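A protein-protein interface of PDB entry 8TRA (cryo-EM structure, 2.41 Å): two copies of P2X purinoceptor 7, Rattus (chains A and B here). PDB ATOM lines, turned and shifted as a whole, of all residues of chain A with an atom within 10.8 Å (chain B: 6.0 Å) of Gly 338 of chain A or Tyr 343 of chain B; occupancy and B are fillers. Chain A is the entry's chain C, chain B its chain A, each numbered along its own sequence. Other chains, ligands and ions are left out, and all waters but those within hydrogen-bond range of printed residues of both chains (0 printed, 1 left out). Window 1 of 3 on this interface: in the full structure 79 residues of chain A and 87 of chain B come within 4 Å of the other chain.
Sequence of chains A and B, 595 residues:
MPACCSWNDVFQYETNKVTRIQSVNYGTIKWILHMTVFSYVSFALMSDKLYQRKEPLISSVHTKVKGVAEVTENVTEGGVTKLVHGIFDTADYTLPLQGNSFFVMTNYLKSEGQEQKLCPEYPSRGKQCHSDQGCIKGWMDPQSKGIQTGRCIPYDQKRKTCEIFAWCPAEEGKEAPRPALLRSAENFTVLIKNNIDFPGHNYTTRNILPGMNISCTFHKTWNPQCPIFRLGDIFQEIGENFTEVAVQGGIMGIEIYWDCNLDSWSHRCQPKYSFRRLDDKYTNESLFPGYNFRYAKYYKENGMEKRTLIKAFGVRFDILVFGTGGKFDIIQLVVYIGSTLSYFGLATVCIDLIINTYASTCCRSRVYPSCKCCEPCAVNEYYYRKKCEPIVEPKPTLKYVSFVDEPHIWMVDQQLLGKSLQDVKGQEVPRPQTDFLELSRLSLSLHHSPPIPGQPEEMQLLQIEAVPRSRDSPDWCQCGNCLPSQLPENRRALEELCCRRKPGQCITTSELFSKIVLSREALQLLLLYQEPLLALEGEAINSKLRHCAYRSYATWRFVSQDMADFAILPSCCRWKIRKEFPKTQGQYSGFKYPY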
ATOM      1  N   VAL A  37     -18.606   5.695  18.883  1.00  0.00           N
ATOM      2  CA  VAL A  37     -18.693   4.816  20.046  1.00  0.00           C
ATOM      3  C   VAL A  37     -18.699   3.357  19.605  1.00  0.00           C
ATOM      4  O   VAL A  37     -17.993   2.515  20.171  1.00  0.00           O
ATOM      5  CB  VAL A  37     -19.939   5.158  20.883  1.00  0.00           C
ATOM      6  CG1 VAL A  37     -20.247   4.042  21.873  1.00  0.00           C
ATOM      7  CG2 VAL A  37     -19.744   6.479  21.608  1.00  0.00           C
ATOM      8  N   VAL A  41     -15.825   0.588  20.494  1.00  0.00           N
ATOM      9  CA  VAL A  41     -16.213  -0.599  21.251  1.00  0.00           C
ATOM     10  C   VAL A  41     -15.832  -1.860  20.488  1.00  0.00           C
ATOM     11  O   VAL A  41     -15.254  -2.800  21.049  1.00  0.00           O
ATOM     12  CB  VAL A  41     -17.720  -0.557  21.566  1.00  0.00           C
ATOM     13  CG1 VAL A  41     -18.236  -1.938  21.943  1.00  0.00           C
ATOM     14  CG2 VAL A  41     -17.998   0.441  22.680  1.00  0.00           C
ATOM     15  N   LEU A  45     -13.113  -4.684  21.596  1.00  0.00           N
ATOM     16  CA  LEU A  45     -13.547  -6.057  21.759  1.00  0.00           C
ATOM     17  C   LEU A  45     -12.710  -6.981  20.906  1.00  0.00           C
ATOM     18  O   LEU A  45     -12.327  -8.058  21.348  1.00  0.00           O
ATOM     19  CB  LEU A  45     -15.018  -6.196  21.386  1.00  0.00           C
ATOM     20  CG  LEU A  45     -15.587  -7.611  21.502  1.00  0.00           C
ATOM     21  CD1 LEU A  45     -15.379  -8.167  22.898  1.00  0.00           C
ATOM     22  CD2 LEU A  45     -17.057  -7.625  21.138  1.00  0.00           C
ATOM     23  N   LEU A  50     -11.976  -9.438  24.218  1.00  0.00           N
ATOM     24  CA  LEU A  50     -12.774  -9.403  25.436  1.00  0.00           C
ATOM     25  C   LEU A  50     -13.963 -10.352  25.387  1.00  0.00           C
ATOM     26  O   LEU A  50     -14.601 -10.572  26.421  1.00  0.00           O
ATOM     27  CB  LEU A  50     -13.251  -7.975  25.700  1.00  0.00           C
ATOM     28  CG  LEU A  50     -12.112  -6.960  25.826  1.00  0.00           C
ATOM     29  CD1 LEU A  50     -12.640  -5.537  25.814  1.00  0.00           C
ATOM     30  CD2 LEU A  50     -11.302  -7.223  27.085  1.00  0.00           C
ATOM     31  N   ASP A 329     -16.561 -17.012  24.896  1.00  0.00           N
ATOM     32  CA  ASP A 329     -17.472 -17.227  26.011  1.00  0.00           C
ATOM     33  C   ASP A 329     -18.635 -16.254  25.888  1.00  0.00           C
ATOM     34  O   ASP A 329     -18.425 -15.054  25.687  1.00  0.00           O
ATOM     35  CB  ASP A 329     -16.760 -17.040  27.354  1.00  0.00           C
ATOM     36  CG  ASP A 329     -17.649 -17.373  28.537  1.00  0.00           C
ATOM     37  OD1 ASP A 329     -18.543 -18.233  28.388  1.00  0.00           O
ATOM     38  OD2 ASP A 329     -17.451 -16.775  29.615  1.00  0.00           O
ATOM     39  N   ILE A 330     -19.858 -16.774  26.012  1.00  0.00           N
ATOM     40  CA  ILE A 330     -21.039 -15.925  25.887  1.00  0.00           C
ATOM     41  C   ILE A 330     -21.133 -14.957  27.060  1.00  0.00           C
ATOM     42  O   ILE A 330     -21.513 -13.791  26.890  1.00  0.00           O
ATOM     43  CB  ILE A 330     -22.307 -16.794  25.757  1.00  0.00           C
ATOM     44  CG1 ILE A 330     -23.522 -15.945  25.356  1.00  0.00           C
ATOM     45  CG2 ILE A 330     -22.588 -17.555  27.050  1.00  0.00           C
ATOM     46  CD1 ILE A 330     -23.378 -15.199  24.040  1.00  0.00           C
ATOM     47  N   ILE A 331     -20.794 -15.417  28.266  1.00  0.00           N
ATOM     48  CA  ILE A 331     -20.940 -14.574  29.450  1.00  0.00           C
ATOM     49  C   ILE A 331     -20.008 -13.370  29.371  1.00  0.00           C
ATOM     50  O   ILE A 331     -20.400 -12.245  29.700  1.00  0.00           O
ATOM     51  CB  ILE A 331     -20.697 -15.401  30.725  1.00  0.00           C
ATOM     52  CG1 ILE A 331     -21.903 -16.302  31.001  1.00  0.00           C
ATOM     53  CG2 ILE A 331     -20.433 -14.486  31.914  1.00  0.00           C
ATOM     54  CD1 ILE A 331     -21.644 -17.388  32.023  1.00  0.00           C
ATOM     55  N   GLN A 332     -18.762 -13.587  28.946  1.00  0.00           N
ATOM     56  CA  GLN A 332     -17.816 -12.479  28.846  1.00  0.00           C
ATOM     57  C   GLN A 332     -18.277 -11.452  27.820  1.00  0.00           C
ATOM     58  O   GLN A 332     -18.203 -10.240  28.063  1.00  0.00           O
ATOM     59  CB  GLN A 332     -16.427 -13.011  28.488  1.00  0.00           C
ATOM     60  CG  GLN A 332     -15.719 -13.720  29.633  1.00  0.00           C
ATOM     61  CD  GLN A 332     -15.374 -12.786  30.775  1.00  0.00           C
ATOM     62  OE1 GLN A 332     -14.365 -12.082  30.735  1.00  0.00           O
ATOM     63  NE2 GLN A 332     -16.215 -12.773  31.804  1.00  0.00           N
ATOM     64  N   LEU A 333     -18.753 -11.917  26.663  1.00  0.00           N
ATOM     65  CA  LEU A 333     -19.248 -10.996  25.643  1.00  0.00           C
ATOM     66  C   LEU A 333     -20.451 -10.213  26.152  1.00  0.00           C
ATOM     67  O   LEU A 333     -20.559  -9.004  25.920  1.00  0.00           O
ATOM     68  CB  LEU A 333     -19.606 -11.770  24.375  1.00  0.00           C
ATOM     69  CG  LEU A 333     -20.221 -10.963  23.228  1.00  0.00           C
ATOM     70  CD1 LEU A 333     -19.228  -9.951  22.684  1.00  0.00           C
ATOM     71  CD2 LEU A 333     -20.699 -11.891  22.125  1.00  0.00           C
ATOM     72  N   VAL A 334     -21.369 -10.891  26.848  1.00  0.00           N
ATOM     73  CA  VAL A 334     -22.542 -10.212  27.389  1.00  0.00           C
ATOM     74  C   VAL A 334     -22.120  -9.153  28.400  1.00  0.00           C
ATOM     75  O   VAL A 334     -22.649  -8.036  28.410  1.00  0.00           O
ATOM     76  CB  VAL A 334     -23.508 -11.237  28.011  1.00  0.00           C
ATOM     77  CG1 VAL A 334     -24.546 -10.540  28.876  1.00  0.00           C
ATOM     78  CG2 VAL A 334     -24.183 -12.055  26.924  1.00  0.00           C
ATOM     79  N   VAL A 335     -21.165  -9.490  29.270  1.00  0.00           N
ATOM     80  CA  VAL A 335     -20.704  -8.538  30.274  1.00  0.00           C
ATOM     81  C   VAL A 335     -20.070  -7.324  29.608  1.00  0.00           C
ATOM     82  O   VAL A 335     -20.326  -6.180  30.000  1.00  0.00           O
ATOM     83  CB  VAL A 335     -19.730  -9.226  31.250  1.00  0.00           C
ATOM     84  CG1 VAL A 335     -18.970  -8.193  32.068  1.00  0.00           C
ATOM     85  CG2 VAL A 335     -20.480 -10.183  32.160  1.00  0.00           C
ATOM     86  N   TYR A 336     -19.229  -7.552  28.597  1.00  0.00           N
ATOM     87  CA  TYR A 336     -18.590  -6.432  27.913  1.00  0.00           C
ATOM     88  C   TYR A 336     -19.619  -5.548  27.218  1.00  0.00           C
ATOM     89  O   TYR A 336     -19.534  -4.313  27.276  1.00  0.00           O
ATOM     90  CB  TYR A 336     -17.563  -6.941  26.903  1.00  0.00           C
ATOM     91  CG  TYR A 336     -16.979  -5.843  26.047  1.00  0.00           C
ATOM     92  CD1 TYR A 336     -15.998  -4.996  26.544  1.00  0.00           C
ATOM     93  CD2 TYR A 336     -17.414  -5.643  24.744  1.00  0.00           C
ATOM     94  CE1 TYR A 336     -15.465  -3.988  25.771  1.00  0.00           C
ATOM     95  CE2 TYR A 336     -16.886  -4.637  23.962  1.00  0.00           C
ATOM     96  CZ  TYR A 336     -15.911  -3.812  24.480  1.00  0.00           C
ATOM     97  OH  TYR A 336     -15.379  -2.807  23.706  1.00  0.00           O
ATOM     98  N   ILE A 337     -20.597  -6.160  26.548  1.00  0.00           N
ATOM     99  CA  ILE A 337     -21.619  -5.380  25.860  1.00  0.00           C
ATOM    100  C   ILE A 337     -22.427  -4.568  26.863  1.00  0.00           C
ATOM    101  O   ILE A 337     -22.743  -3.398  26.624  1.00  0.00           O
ATOM    102  CB  ILE A 337     -22.520  -6.299  25.015  1.00  0.00           C
ATOM    103  CG1 ILE A 337     -21.753  -6.804  23.791  1.00  0.00           C
ATOM    104  CG2 ILE A 337     -23.781  -5.559  24.583  1.00  0.00           C
ATOM    105  CD1 ILE A 337     -22.405  -7.981  23.100  1.00  0.00           C
ATOM    106  N   GLY A 338     -22.785  -5.175  27.995  1.00  0.00           N
ATOM    107  CA  GLY A 338     -23.497  -4.432  29.020  1.00  0.00           C
ATOM    108  C   GLY A 338     -22.683  -3.276  29.568  1.00  0.00           C
ATOM    109  O   GLY A 338     -23.216  -2.196  29.829  1.00  0.00           O
ATOM    110  N   SER A 339     -21.380  -3.491  29.750  1.00  0.00           N
ATOM    111  CA  SER A 339     -20.517  -2.419  30.235  1.00  0.00           C
ATOM    112  C   SER A 339     -20.458  -1.267  29.241  1.00  0.00           C
ATOM    113  O   SER A 339     -20.486  -0.096  29.635  1.00  0.00           O
ATOM    114  CB  SER A 339     -19.113  -2.961  30.507  1.00  0.00           C
ATOM    115  OG  SER A 339     -18.450  -3.290  29.300  1.00  0.00           O
ATOM    116  N   THR A 340     -20.377  -1.576  27.948  1.00  0.00           N
ATOM    117  CA  THR A 340     -20.201  -0.547  26.930  1.00  0.00           C
ATOM    118  C   THR A 340     -21.515   0.036  26.414  1.00  0.00           C
ATOM    119  O   THR A 340     -21.482   1.004  25.649  1.00  0.00           O
ATOM    120  CB  THR A 340     -19.404  -1.106  25.746  1.00  0.00           C
ATOM    121  OG1 THR A 340     -19.977  -2.350  25.323  1.00  0.00           O
ATOM    122  CG2 THR A 340     -17.951  -1.326  26.139  1.00  0.00           C
ATOM    123  N   LEU A 341     -22.663  -0.523  26.808  1.00  0.00           N
ATOM    124  CA  LEU A 341     -23.937  -0.019  26.303  1.00  0.00           C
ATOM    125  C   LEU A 341     -24.164   1.436  26.697  1.00  0.00           C
ATOM    126  O   LEU A 341     -24.628   2.242  25.880  1.00  0.00           O
ATOM    127  CB  LEU A 341     -25.084  -0.890  26.815  1.00  0.00           C
ATOM    128  CG  LEU A 341     -25.509  -2.065  25.935  1.00  0.00           C
ATOM    129  CD1 LEU A 341     -26.480  -2.967  26.684  1.00  0.00           C
ATOM    130  CD2 LEU A 341     -26.127  -1.581  24.633  1.00  0.00           C
ATOM    131  N   SER A 342     -23.849   1.795  27.942  1.00  0.00           N
ATOM    132  CA  SER A 342     -24.157   3.136  28.427  1.00  0.00           C
ATOM    133  C   SER A 342     -23.415   4.222  27.657  1.00  0.00           C
ATOM    134  O   SER A 342     -23.813   5.390  27.722  1.00  0.00           O
ATOM    135  CB  SER A 342     -23.830   3.244  29.916  1.00  0.00           C
ATOM    136  OG  SER A 342     -24.864   2.685  30.706  1.00  0.00           O
ATOM    137  N   TYR A 343     -22.351   3.870  26.936  1.00  0.00           N
ATOM    138  CA  TYR A 343     -21.604   4.861  26.174  1.00  0.00           C
ATOM    139  C   TYR A 343     -22.368   5.370  24.958  1.00  0.00           C
ATOM    140  O   TYR A 343     -21.958   6.378  24.372  1.00  0.00           O
ATOM    141  CB  TYR A 343     -20.262   4.278  25.728  1.00  0.00           C
ATOM    142  CG  TYR A 343     -19.187   4.342  26.789  1.00  0.00           C
ATOM    143  CD1 TYR A 343     -18.777   5.559  27.318  1.00  0.00           C
ATOM    144  CD2 TYR A 343     -18.583   3.185  27.261  1.00  0.00           C
ATOM    145  CE1 TYR A 343     -17.796   5.621  28.286  1.00  0.00           C
ATOM    146  CE2 TYR A 343     -17.601   3.240  28.230  1.00  0.00           C
ATOM    147  CZ  TYR A 343     -17.211   4.459  28.739  1.00  0.00           C
ATOM    148  OH  TYR A 343     -16.232   4.517  29.703  1.00  0.00           O
ATOM    149  N   PHE A 344     -23.456   4.708  24.567  1.00  0.00           N
ATOM    150  CA  PHE A 344     -24.244   5.153  23.426  1.00  0.00           C
ATOM    151  C   PHE A 344     -25.161   6.324  23.759  1.00  0.00           C
ATOM    152  O   PHE A 344     -25.778   6.884  22.846  1.00  0.00           O
ATOM    153  CB  PHE A 344     -25.069   3.987  22.876  1.00  0.00           C
ATOM    154  CG  PHE A 344     -24.257   2.989  22.101  1.00  0.00           C
ATOM    155  CD1 PHE A 344     -23.820   3.279  20.820  1.00  0.00           C
ATOM    156  CD2 PHE A 344     -23.928   1.765  22.655  1.00  0.00           C
ATOM    157  CE1 PHE A 344     -23.072   2.364  20.104  1.00  0.00           C
ATOM    158  CE2 PHE A 344     -23.178   0.846  21.945  1.00  0.00           C
ATOM    159  CZ  PHE A 344     -22.750   1.148  20.668  1.00  0.00           C
ATOM    160  N   GLY A 345     -25.267   6.701  25.031  1.00  0.00           N
ATOM    161  CA  GLY A 345     -25.982   7.896  25.422  1.00  0.00           C
ATOM    162  C   GLY A 345     -25.180   9.170  25.322  1.00  0.00           C
ATOM    163  O   GLY A 345     -25.667  10.238  25.707  1.00  0.00           O
ATOM    164  N   VAL B  37     -34.292 -11.137  31.460  1.00  0.00           N
ATOM    165  CA  VAL B  37     -33.004 -10.491  31.688  1.00  0.00           C
ATOM    166  C   VAL B  37     -32.511 -10.782  33.100  1.00  0.00           C
ATOM    167  O   VAL B  37     -31.339 -11.119  33.312  1.00  0.00           O
ATOM    168  CB  VAL B  37     -33.112  -8.977  31.429  1.00  0.00           C
ATOM    169  CG1 VAL B  37     -31.907  -8.244  32.001  1.00  0.00           C
ATOM    170  CG2 VAL B  37     -33.247  -8.702  29.939  1.00  0.00           C
ATOM    171  N   VAL B  41     -29.131 -12.876  34.058  1.00  0.00           N
ATOM    172  CA  VAL B  41     -28.087 -12.200  34.823  1.00  0.00           C
ATOM    173  C   VAL B  41     -27.773 -12.981  36.093  1.00  0.00           C
ATOM    174  O   VAL B  41     -26.606 -13.217  36.428  1.00  0.00           O
ATOM    175  CB  VAL B  41     -28.511 -10.752  35.134  1.00  0.00           C
ATOM    176  CG1 VAL B  41     -27.686 -10.176  36.274  1.00  0.00           C
ATOM    177  CG2 VAL B  41     -28.383  -9.887  33.890  1.00  0.00           C
ATOM    178  N   GLY B 338     -23.426  -3.270  37.680  1.00  0.00           N
ATOM    179  CA  GLY B 338     -23.401  -2.093  36.829  1.00  0.00           C
ATOM    180  C   GLY B 338     -23.313  -2.447  35.358  1.00  0.00           C
ATOM    181  O   GLY B 338     -23.950  -1.809  34.516  1.00  0.00           O
ATOM    182  N   SER B 339     -22.520  -3.467  35.028  1.00  0.00           N
ATOM    183  CA  SER B 339     -22.411  -3.897  33.639  1.00  0.00           C
ATOM    184  C   SER B 339     -23.743  -4.420  33.117  1.00  0.00           C
ATOM    185  O   SER B 339     -24.123  -4.139  31.975  1.00  0.00           O
ATOM    186  CB  SER B 339     -21.328  -4.969  33.509  1.00  0.00           C
ATOM    187  OG  SER B 339     -21.736  -6.184  34.117  1.00  0.00           O
ATOM    188  N   THR B 340     -24.465  -5.182  33.937  1.00  0.00           N
ATOM    189  CA  THR B 340     -25.697  -5.822  33.489  1.00  0.00           C
ATOM    190  C   THR B 340     -26.939  -4.952  33.668  1.00  0.00           C
ATOM    191  O   THR B 340     -28.015  -5.341  33.204  1.00  0.00           O
ATOM    192  CB  THR B 340     -25.903  -7.147  34.233  1.00  0.00           C
ATOM    193  OG1 THR B 340     -25.753  -6.937  35.643  1.00  0.00           O
ATOM    194  CG2 THR B 340     -24.894  -8.183  33.765  1.00  0.00           C
ATOM    195  N   LEU B 341     -26.823  -3.795  34.324  1.00  0.00           N
ATOM    196  CA  LEU B 341     -27.996  -2.957  34.550  1.00  0.00           C
ATOM    197  C   LEU B 341     -28.619  -2.492  33.238  1.00  0.00           C
ATOM    198  O   LEU B 341     -29.849  -2.492  33.094  1.00  0.00           O
ATOM    199  CB  LEU B 341     -27.620  -1.750  35.411  1.00  0.00           C
ATOM    200  CG  LEU B 341     -27.775  -1.904  36.925  1.00  0.00           C
ATOM    201  CD1 LEU B 341     -27.138  -0.725  37.646  1.00  0.00           C
ATOM    202  CD2 LEU B 341     -29.236  -2.044  37.317  1.00  0.00           C
ATOM    203  N   SER B 342     -27.792  -2.090  32.271  1.00  0.00           N
ATOM    204  CA  SER B 342     -28.321  -1.515  31.040  1.00  0.00           C
ATOM    205  C   SER B 342     -29.170  -2.502  30.249  1.00  0.00           C
ATOM    206  O   SER B 342     -29.941  -2.079  29.380  1.00  0.00           O
ATOM    207  CB  SER B 342     -27.176  -1.004  30.165  1.00  0.00           C
ATOM    208  OG  SER B 342     -26.728   0.265  30.605  1.00  0.00           O
ATOM    209  N   TYR B 343     -29.049  -3.801  30.524  1.00  0.00           N
ATOM    210  CA  TYR B 343     -29.839  -4.792  29.806  1.00  0.00           C
ATOM    211  C   TYR B 343     -31.313  -4.761  30.185  1.00  0.00           C
ATOM    212  O   TYR B 343     -32.126  -5.372  29.483  1.00  0.00           O
ATOM    213  CB  TYR B 343     -29.275  -6.192  30.056  1.00  0.00           C
ATOM    214  CG  TYR B 343     -28.102  -6.545  29.171  1.00  0.00           C
ATOM    215  CD1 TYR B 343     -28.229  -6.561  27.789  1.00  0.00           C
ATOM    216  CD2 TYR B 343     -26.866  -6.859  29.718  1.00  0.00           C
ATOM    217  CE1 TYR B 343     -27.162  -6.882  26.978  1.00  0.00           C
ATOM    218  CE2 TYR B 343     -25.792  -7.180  28.914  1.00  0.00           C
ATOM    219  CZ  TYR B 343     -25.944  -7.191  27.545  1.00  0.00           C
ATOM    220  OH  TYR B 343     -24.876  -7.512  26.740  1.00  0.00           O
ATOM    221  N   PHE B 344     -31.679  -4.072  31.265  1.00  0.00           N
ATOM    222  CA  PHE B 344     -33.074  -3.983  31.672  1.00  0.00           C
ATOM    223  C   PHE B 344     -33.869  -2.978  30.848  1.00  0.00           C
ATOM    224  O   PHE B 344     -35.093  -2.909  31.000  1.00  0.00           O
ATOM    225  CB  PHE B 344     -33.162  -3.622  33.157  1.00  0.00           C
ATOM    226  CG  PHE B 344     -32.825  -4.763  34.073  1.00  0.00           C
ATOM    227  CD1 PHE B 344     -33.726  -5.795  34.274  1.00  0.00           C
ATOM    228  CD2 PHE B 344     -31.607  -4.806  34.730  1.00  0.00           C
ATOM    229  CE1 PHE B 344     -33.417  -6.848  35.115  1.00  0.00           C
ATOM    230  CE2 PHE B 344     -31.294  -5.856  35.571  1.00  0.00           C
ATOM    231  CZ  PHE B 344     -32.200  -6.878  35.762  1.00  0.00           C
ATOM    232  N   GLY B 345     -33.210  -2.202  29.990  1.00  0.00           N
ATOM    233  CA  GLY B 345     -33.892  -1.336  29.053  1.00  0.00           C
ATOM    234  C   GLY B 345     -34.341  -2.015  27.783  1.00  0.00           C
ATOM    235  O   GLY B 345     -34.863  -1.352  26.880  1.00  0.00           O
ATOM    236  N   LEU B 346     -34.138  -3.332  27.686  1.00  0.00           N
ATOM    237  CA  LEU B 346     -34.531  -4.062  26.488  1.00  0.00           C
ATOM    238  C   LEU B 346     -36.036  -3.995  26.269  1.00  0.00           C
ATOM    239  O   LEU B 346     -36.499  -3.852  25.132  1.00  0.00           O
ATOM    240  CB  LEU B 346     -34.074  -5.516  26.592  1.00  0.00           C
ATOM    241  CG  LEU B 346     -34.270  -6.376  25.341  1.00  0.00           C
ATOM    242  CD1 LEU B 346     -33.170  -6.104  24.329  1.00  0.00           C
ATOM    243  CD2 LEU B 346     -34.316  -7.848  25.708  1.00  0.00           C
ATOM    244  N   ALA B 347     -36.819  -4.114  27.343  1.00  0.00           N
ATOM    245  CA  ALA B 347     -38.270  -4.040  27.208  1.00  0.00           C
ATOM    246  C   ALA B 347     -38.696  -2.690  26.650  1.00  0.00           C
ATOM    247  O   ALA B 347     -39.509  -2.616  25.719  1.00  0.00           O
ATOM    248  CB  ALA B 347     -38.932  -4.293  28.562  1.00  0.00           C
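OG of Ser 342 of chain A is in hydrogen-bond range of OG of Ser 342 of chain B (3.1 Å). The backbone carbonyl oxygen (O) of Val 334 of chain A sits at hydrogen-bond distance from the side-chain hydroxyl (OH) of Tyr 343 of chain B (2.8 Å). N of Gly 338 of chain A sits at hydrogen-bond distance from OH of Tyr 343 of chain B, 3.4 Å away. The backbone carbonyl oxygen of Gly 338 of chain A sits close to the backbone carbonyl oxygen of Ser 339 of chain B.
OG of Ser 339 of chain A lies within hydrogen-bond range of O of Tyr 336 of chain A (2.5 Å). The side-chain hydroxyl of Thr 340 of chain A is in hydrogen-bond range of the backbone carbonyl oxygen of Ile 337 of chain A (3.2 Å).
Among the printed residues, pairs that only touch across the chains: Val 335 of chain A with Ser 339 of chain B (3.8 Å), Ile 337 of chain A with Tyr 343 of chain B (3.1 Å), Ser 339 of chain A with Ser 339 of chain B (3.6 Å), Leu 341 of chain A with Ser 342 of chain B (3.95 Å) and Leu 341 of chain A with Tyr 343 of chain B (3.98 Å).
Leu 50 of chain A touches none of the printed residues of chain B. Of the printed residues of chain B, Val 335 of chain A touches Ser 339 (3.8 Å). Of chain B, only Ser 339 (2.9 Å) and Tyr 343 (3.4 Å) come within 4 Å of Gly 338 of chain A. Of the printed residues of chain B, Ser 339 of chain A touches Ser 339 (3.6 Å). Printed residues of chain B within 4 Å of Leu 341 of chain A: Ser 342 and Tyr 343. Printed residues of chain B within 4 Å of Ser 342 of chain A: Ser 342 (3.1 Å). Tyr 343 of chain A touches none of the printed residues of chain B. No residue of chain A comes within 4 Å of Val 37 of chain B. Printed residues of chain A within 4 Å of Ser 339 of chain B: Val 335, Gly 338 and Ser 339. No residue of chain A comes within 4 Å of Thr 340 of chain B. Of the printed residues of chain A, Ser 342 of chain B touches Leu 341 (3.95 Å) and Ser 342 (3.1 Å). Of the printed residues of chain A, Tyr 343 of chain B touches Val 334 (2.8 Å), Ile 337 (3.1 Å), Gly 338 (3.4 Å) and Leu 341 (3.98 Å). Phe 344 of chain B touches none of the printed residues of chain A. No residue of chain A comes within 4 Å of Gly 345 of chain B.
Hydrophobic or aromatic side chains of chain A that line the printed part of chain B: Val 334, Val 335, Ile 337 and Leu 341.
Gly 338 of chain A touches Ser 339 of chain B, but with the chains exchanged Ser 339 of chain A does not touch Gly 338 of chain B (5.5 Å). Gly 338 of chain A touches Tyr 343 of chain B, but with the chains exchanged Tyr 343 of chain A does not touch Gly 338 of chain B (9.6 Å). Ser 339 of chain A touches its own counterpart, Ser 339 of chain B. Leu 341 of chain A touches Ser 342 of chain B, but with the chains exchanged Ser 342 of chain A does not touch Leu 341 of chain B (6.9 Å).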
